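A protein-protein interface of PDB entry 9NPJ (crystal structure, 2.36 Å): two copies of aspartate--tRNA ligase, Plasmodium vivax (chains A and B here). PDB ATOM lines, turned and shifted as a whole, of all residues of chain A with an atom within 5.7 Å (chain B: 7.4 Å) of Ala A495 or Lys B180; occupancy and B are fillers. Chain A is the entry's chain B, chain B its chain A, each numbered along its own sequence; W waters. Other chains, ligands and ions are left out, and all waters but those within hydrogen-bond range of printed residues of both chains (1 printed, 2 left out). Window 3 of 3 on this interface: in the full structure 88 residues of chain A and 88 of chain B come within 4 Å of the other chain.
Ile A491 touches none of the printed residues of chain B. Ala A495 touches just these residues of chain B: Thr B178, Ala B179 and Lys B180. Of the printed residues of chain B, Ser A497 touches Glu B142 (2.9 Å), Ser B176 (3.3 Å) and Thr B178 (3.9 Å). Printed residues of chain A within 4 Å of Thr B178: Ala A495 (3.7 Å), Tyr A496 (3.7 Å) and Ser A497 (3.9 Å). Of the printed residues of chain A, Lys B180 touches Asp A492, Ala A495 and Tyr A496. Of the printed residues of chain A, Glu B181 touches Tyr A496. Printed residues of chain A within 4 Å of Pro B183: Tyr A496 (3.96 Å). Asn B210 touches none of the printed residues of chain A. Printed residues of chain A within 4 Å of Arg B216: Tyr A496.
No position is printed for both chains.
The side-chain amino group (NZ) of Lys B180 lies within salt-bridge range of the side-chain carboxylate (OD2) of Asp A492 (2.9 Å). The backbone carbonyl oxygen of Tyr A496 sits at hydrogen-bond distance from the guanidinium group of Arg B216. N of Ala B179 sits at hydrogen-bond distance from O of Ala A495, 2.9 Å away. The backbone carbonyl oxygen (O) of Glu B142 is in hydrogen-bond range of the side-chain hydroxyl (OG) of Ser A497 (2.9 Å). The backbone NH (N) of Lys B180 sits at hydrogen-bond distance from the backbone carbonyl oxygen (O) of Ala A495, 3.4 Å away.
Water W1 lies within hydrogen-bond range of the backbone carbonyl oxygen (O) of Ser A493 (2.5 Å), the guanidinium group (NH2) of Arg B216 (2.7 Å), the backbone carbonyl oxygen (O) of Ser A497 (2.7 Å) and the backbone NH (N) of Tyr A496 (2.9 Å).
Of the 8 printed residues of chain A, 5 touch a printed residue of chain B.
Among the printed residues, merely in contact across the chains: Val A470 with Ala B179, Ala A495 with Thr B178, Tyr A496 with Glu B142, Tyr A496 with Thr B178, Tyr A496 with Lys B180, Tyr A496 with Glu B181, Tyr A496 with Leu B182, Tyr A496 with Pro B183, Ser A497 with Ser B176 and Ser A497 with Thr B178.
The side-chain carboxylate (OE1) of Glu B142 lies within salt-bridge range of the guanidinium group (NH1) of Arg B216. The side-chain hydroxyl of Thr B178 is in hydrogen-bond range of the backbone carbonyl oxygen of Leu B141 (2.6 Å). The side-chain carboxylate (OD1) of Asp A492 is in hydrogen-bond range of the side-chain hydroxyl (OH) of Tyr A496 (2.7 Å).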
ATOM      1  N   VAL A 470     -14.107  16.067 -32.589  1.00  0.00           N
ATOM      2  CA  VAL A 470     -13.638  16.895 -33.702  1.00  0.00           C
ATOM      3  C   VAL A 470     -14.021  16.290 -35.049  1.00  0.00           C
ATOM      4  O   VAL A 470     -14.307  17.024 -36.000  1.00  0.00           O
ATOM      5  CB  VAL A 470     -12.120  17.147 -33.624  1.00  0.00           C
ATOM      6  CG1 VAL A 470     -11.344  15.887 -33.977  1.00  0.00           C
ATOM      7  CG2 VAL A 470     -11.726  18.299 -34.551  1.00  0.00           C
ATOM      8  N   ILE A 491     -12.371  24.852 -34.677  1.00  0.00           N
ATOM      9  CA  ILE A 491     -12.260  23.407 -34.855  1.00  0.00           C
ATOM     10  C   ILE A 491     -11.048  22.868 -34.105  1.00  0.00           C
ATOM     11  O   ILE A 491     -11.114  21.847 -33.410  1.00  0.00           O
ATOM     12  CB  ILE A 491     -12.161  23.066 -36.352  1.00  0.00           C
ATOM     13  CG1 ILE A 491     -13.455  23.437 -37.070  1.00  0.00           C
ATOM     14  CG2 ILE A 491     -11.801  21.600 -36.547  1.00  0.00           C
ATOM     15  CD1 ILE A 491     -13.322  23.354 -38.562  1.00  0.00           C
ATOM     16  N   ASP A 492      -9.912  23.539 -34.261  1.00  0.00           N
ATOM     17  CA  ASP A 492      -8.669  23.001 -33.739  1.00  0.00           C
ATOM     18  C   ASP A 492      -8.730  22.845 -32.230  1.00  0.00           C
ATOM     19  O   ASP A 492      -8.079  21.958 -31.667  1.00  0.00           O
ATOM     20  CB  ASP A 492      -7.506  23.906 -34.163  1.00  0.00           C
ATOM     21  CG  ASP A 492      -6.188  23.172 -34.217  1.00  0.00           C
ATOM     22  OD1 ASP A 492      -5.304  23.491 -33.380  1.00  0.00           O
ATOM     23  OD2 ASP A 492      -6.048  22.258 -35.074  1.00  0.00           O
ATOM     24  N   SER A 493      -9.529  23.677 -31.560  1.00  0.00           N
ATOM     25  CA  SER A 493      -9.583  23.621 -30.108  1.00  0.00           C
ATOM     26  C   SER A 493     -10.222  22.338 -29.599  1.00  0.00           C
ATOM     27  O   SER A 493     -10.115  22.072 -28.402  1.00  0.00           O
ATOM     28  CB  SER A 493     -10.326  24.846 -29.551  1.00  0.00           C
ATOM     29  OG  SER A 493     -11.730  24.701 -29.698  1.00  0.00           O
ATOM     30  N   PHE A 494     -10.882  21.560 -30.467  1.00  0.00           N
ATOM     31  CA  PHE A 494     -11.450  20.255 -30.130  1.00  0.00           C
ATOM     32  C   PHE A 494     -10.490  19.101 -30.394  1.00  0.00           C
ATOM     33  O   PHE A 494     -10.844  17.949 -30.116  1.00  0.00           O
ATOM     34  CB  PHE A 494     -12.733  19.977 -30.935  1.00  0.00           C
ATOM     35  CG  PHE A 494     -13.846  20.954 -30.698  1.00  0.00           C
ATOM     36  CD1 PHE A 494     -13.853  22.197 -31.340  1.00  0.00           C
ATOM     37  CD2 PHE A 494     -14.913  20.618 -29.865  1.00  0.00           C
ATOM     38  CE1 PHE A 494     -14.893  23.102 -31.132  1.00  0.00           C
ATOM     39  CE2 PHE A 494     -15.957  21.508 -29.640  1.00  0.00           C
ATOM     40  CZ  PHE A 494     -15.949  22.763 -30.268  1.00  0.00           C
ATOM     41  N   ALA A 495      -9.309  19.365 -30.963  1.00  0.00           N
ATOM     42  CA  ALA A 495      -8.473  18.290 -31.492  1.00  0.00           C
ATOM     43  C   ALA A 495      -7.475  17.764 -30.474  1.00  0.00           C
ATOM     44  O   ALA A 495      -6.712  16.842 -30.795  1.00  0.00           O
ATOM     45  CB  ALA A 495      -7.734  18.752 -32.758  1.00  0.00           C
ATOM     46  N   TYR A 496      -7.467  18.325 -29.261  1.00  0.00           N
ATOM     47  CA  TYR A 496      -6.641  17.802 -28.178  1.00  0.00           C
ATOM     48  C   TYR A 496      -7.550  17.388 -27.028  1.00  0.00           C
ATOM     49  O   TYR A 496      -7.298  17.724 -25.862  1.00  0.00           O
ATOM     50  CB  TYR A 496      -5.598  18.839 -27.760  1.00  0.00           C
ATOM     51  CG  TYR A 496      -5.052  19.588 -28.959  1.00  0.00           C
ATOM     52  CD1 TYR A 496      -4.101  19.003 -29.804  1.00  0.00           C
ATOM     53  CD2 TYR A 496      -5.516  20.863 -29.272  1.00  0.00           C
ATOM     54  CE1 TYR A 496      -3.610  19.680 -30.902  1.00  0.00           C
ATOM     55  CE2 TYR A 496      -5.035  21.553 -30.365  1.00  0.00           C
ATOM     56  CZ  TYR A 496      -4.083  20.954 -31.183  1.00  0.00           C
ATOM     57  OH  TYR A 496      -3.618  21.643 -32.275  1.00  0.00           O
ATOM     58  N   SER A 497      -8.630  16.669 -27.377  1.00  0.00           N
ATOM     59  CA  SER A 497      -9.655  16.194 -26.451  1.00  0.00           C
ATOM     60  C   SER A 497     -10.701  17.276 -26.194  1.00  0.00           C
ATOM     61  O   SER A 497     -10.383  18.474 -26.195  1.00  0.00           O
ATOM     62  CB  SER A 497      -9.052  15.737 -25.119  1.00  0.00           C
ATOM     63  OG  SER A 497      -8.919  16.835 -24.212  1.00  0.00           O
ATOM     64  N   PRO B 140      -2.597   9.132 -26.056  1.00  0.00           N
ATOM     65  CA  PRO B 140      -1.876  10.404 -26.205  1.00  0.00           C
ATOM     66  C   PRO B 140      -2.236  11.401 -25.107  1.00  0.00           C
ATOM     67  O   PRO B 140      -3.348  11.405 -24.562  1.00  0.00           O
ATOM     68  CB  PRO B 140      -2.324  10.899 -27.588  1.00  0.00           C
ATOM     69  CG  PRO B 140      -3.745  10.331 -27.731  1.00  0.00           C
ATOM     70  CD  PRO B 140      -3.705   8.980 -27.023  1.00  0.00           C
ATOM     71  N   LEU B 141      -1.253  12.248 -24.781  1.00  0.00           N
ATOM     72  CA  LEU B 141      -1.425  13.287 -23.776  1.00  0.00           C
ATOM     73  C   LEU B 141      -2.676  14.108 -24.061  1.00  0.00           C
ATOM     74  O   LEU B 141      -3.085  14.286 -25.211  1.00  0.00           O
ATOM     75  CB  LEU B 141      -0.198  14.205 -23.728  1.00  0.00           C
ATOM     76  CG  LEU B 141       1.135  13.500 -23.456  1.00  0.00           C
ATOM     77  CD1 LEU B 141       2.306  14.488 -23.312  1.00  0.00           C
ATOM     78  CD2 LEU B 141       1.026  12.594 -22.243  1.00  0.00           C
ATOM     79  N   GLU B 142      -3.280  14.611 -22.986  1.00  0.00           N
ATOM     80  CA  GLU B 142      -4.454  15.470 -22.942  1.00  0.00           C
ATOM     81  C   GLU B 142      -5.748  14.690 -23.139  1.00  0.00           C
ATOM     82  O   GLU B 142      -6.815  15.289 -23.054  1.00  0.00           O
ATOM     83  CB  GLU B 142      -4.392  16.615 -23.967  1.00  0.00           C
ATOM     84  CG  GLU B 142      -3.310  17.653 -23.635  1.00  0.00           C
ATOM     85  CD  GLU B 142      -3.493  18.297 -22.248  1.00  0.00           C
ATOM     86  OE1 GLU B 142      -4.461  19.113 -22.053  1.00  0.00           O
ATOM     87  OE2 GLU B 142      -2.652  17.985 -21.365  1.00  0.00           O
ATOM     88  N   SER B 176     -12.559  10.748 -24.467  1.00  0.00           N
ATOM     89  CA  SER B 176     -12.168  11.651 -25.552  1.00  0.00           C
ATOM     90  C   SER B 176     -10.670  11.547 -25.818  1.00  0.00           C
ATOM     91  O   SER B 176      -9.858  11.947 -24.971  1.00  0.00           O
ATOM     92  CB  SER B 176     -12.548  13.095 -25.235  1.00  0.00           C
ATOM     93  OG  SER B 176     -12.082  13.964 -26.257  1.00  0.00           O
ATOM     94  N   LYS B 177     -10.316  11.051 -27.001  1.00  0.00           N
ATOM     95  CA  LYS B 177      -8.922  10.848 -27.384  1.00  0.00           C
ATOM     96  C   LYS B 177      -8.391  12.061 -28.149  1.00  0.00           C
ATOM     97  O   LYS B 177      -9.005  12.500 -29.128  1.00  0.00           O
ATOM     98  CB  LYS B 177      -8.782   9.590 -28.252  1.00  0.00           C
ATOM     99  CG  LYS B 177      -7.324   9.159 -28.488  1.00  0.00           C
ATOM    100  CD  LYS B 177      -7.186   8.121 -29.597  1.00  0.00           C
ATOM    101  CE  LYS B 177      -7.449   8.759 -30.961  1.00  0.00           C
ATOM    102  NZ  LYS B 177      -7.010   7.891 -32.110  1.00  0.00           N
ATOM    103  N   THR B 178      -7.249  12.589 -27.714  1.00  0.00           N
ATOM    104  CA  THR B 178      -6.535  13.591 -28.502  1.00  0.00           C
ATOM    105  C   THR B 178      -6.359  13.119 -29.943  1.00  0.00           C
ATOM    106  O   THR B 178      -5.880  12.009 -30.182  1.00  0.00           O
ATOM    107  CB  THR B 178      -5.165  13.851 -27.875  1.00  0.00           C
ATOM    108  OG1 THR B 178      -5.349  14.398 -26.566  1.00  0.00           O
ATOM    109  CG2 THR B 178      -4.337  14.795 -28.742  1.00  0.00           C
ATOM    110  N   ALA B 179      -6.731  13.968 -30.909  1.00  0.00           N
ATOM    111  CA  ALA B 179      -6.757  13.555 -32.313  1.00  0.00           C
ATOM    112  C   ALA B 179      -5.526  13.981 -33.110  1.00  0.00           C
ATOM    113  O   ALA B 179      -5.354  13.521 -34.245  1.00  0.00           O
ATOM    114  CB  ALA B 179      -8.004  14.107 -33.012  1.00  0.00           C
ATOM    115  N   LYS B 180      -4.658  14.811 -32.543  1.00  0.00           N
ATOM    116  CA  LYS B 180      -3.649  15.519 -33.314  1.00  0.00           C
ATOM    117  C   LYS B 180      -2.463  15.845 -32.411  1.00  0.00           C
ATOM    118  O   LYS B 180      -2.620  16.071 -31.208  1.00  0.00           O
ATOM    119  CB  LYS B 180      -4.279  16.787 -33.924  1.00  0.00           C
ATOM    120  CG  LYS B 180      -3.315  17.854 -34.392  1.00  0.00           C
ATOM    121  CD  LYS B 180      -4.067  18.945 -35.138  1.00  0.00           C
ATOM    122  CE  LYS B 180      -3.159  20.129 -35.462  1.00  0.00           C
ATOM    123  NZ  LYS B 180      -3.809  21.044 -36.448  1.00  0.00           N
ATOM    124  N   GLU B 181      -1.272  15.868 -33.003  1.00  0.00           N
ATOM    125  CA  GLU B 181      -0.066  16.211 -32.261  1.00  0.00           C
ATOM    126  C   GLU B 181      -0.188  17.618 -31.684  1.00  0.00           C
ATOM    127  O   GLU B 181      -0.610  18.549 -32.376  1.00  0.00           O
ATOM    128  CB  GLU B 181       1.153  16.092 -33.189  1.00  0.00           C
ATOM    129  CG  GLU B 181       2.481  16.605 -32.632  1.00  0.00           C
ATOM    130  CD  GLU B 181       3.636  16.479 -33.655  1.00  0.00           C
ATOM    131  OE1 GLU B 181       4.822  16.458 -33.242  1.00  0.00           O
ATOM    132  OE2 GLU B 181       3.356  16.399 -34.875  1.00  0.00           O
ATOM    133  N   LEU B 182       0.171  17.768 -30.407  1.00  0.00           N
ATOM    134  CA  LEU B 182       0.085  19.066 -29.760  1.00  0.00           C
ATOM    135  C   LEU B 182       1.074  20.053 -30.382  1.00  0.00           C
ATOM    136  O   LEU B 182       2.159  19.667 -30.816  1.00  0.00           O
ATOM    137  CB  LEU B 182       0.340  18.943 -28.254  1.00  0.00           C
ATOM    138  CG  LEU B 182      -0.968  18.813 -27.439  1.00  0.00           C
ATOM    139  CD1 LEU B 182      -1.443  17.366 -27.373  1.00  0.00           C
ATOM    140  CD2 LEU B 182      -0.853  19.393 -26.046  1.00  0.00           C
ATOM    141  N   PRO B 183       0.723  21.340 -30.432  1.00  0.00           N
ATOM    142  CA  PRO B 183       1.640  22.328 -31.038  1.00  0.00           C
ATOM    143  C   PRO B 183       2.914  22.523 -30.248  1.00  0.00           C
ATOM    144  O   PRO B 183       3.900  23.018 -30.800  1.00  0.00           O
ATOM    145  CB  PRO B 183       0.806  23.618 -31.058  1.00  0.00           C
ATOM    146  CG  PRO B 183      -0.150  23.442 -29.887  1.00  0.00           C
ATOM    147  CD  PRO B 183      -0.489  21.967 -29.871  1.00  0.00           C
ATOM    148  N   ASN B 210      -2.094  29.139 -30.653  1.00  0.00           N
ATOM    149  CA  ASN B 210      -2.639  27.891 -30.142  1.00  0.00           C
ATOM    150  C   ASN B 210      -3.182  28.121 -28.754  1.00  0.00           C
ATOM    151  O   ASN B 210      -2.817  27.406 -27.813  1.00  0.00           O
ATOM    152  CB  ASN B 210      -1.574  26.813 -30.125  1.00  0.00           C
ATOM    153  CG  ASN B 210      -1.144  26.458 -31.503  1.00  0.00           C
ATOM    154  OD1 ASN B 210      -1.887  25.780 -32.204  1.00  0.00           O
ATOM    155  ND2 ASN B 210       0.030  26.948 -31.934  1.00  0.00           N
ATOM    156  N   ARG B 216      -4.087  26.064 -20.981  1.00  0.00           N
ATOM    157  CA  ARG B 216      -4.066  24.931 -20.062  1.00  0.00           C
ATOM    158  C   ARG B 216      -2.899  24.941 -19.085  1.00  0.00           C
ATOM    159  O   ARG B 216      -2.898  24.107 -18.171  1.00  0.00           O
ATOM    160  CB  ARG B 216      -4.037  23.613 -20.834  1.00  0.00           C
ATOM    161  CG  ARG B 216      -5.151  23.521 -21.828  1.00  0.00           C
ATOM    162  CD  ARG B 216      -5.075  22.282 -22.649  1.00  0.00           C
ATOM    163  NE  ARG B 216      -5.993  22.367 -23.777  1.00  0.00           N
ATOM    164  CZ  ARG B 216      -6.387  21.326 -24.494  1.00  0.00           C
ATOM    165  NH1 ARG B 216      -6.000  20.094 -24.188  1.00  0.00           N
ATOM    166  NH2 ARG B 216      -7.175  21.527 -25.549  1.00  0.00           N
HETATM  167  O   HOH W   1      -8.699  20.236 -27.382  1.00  0.00           O
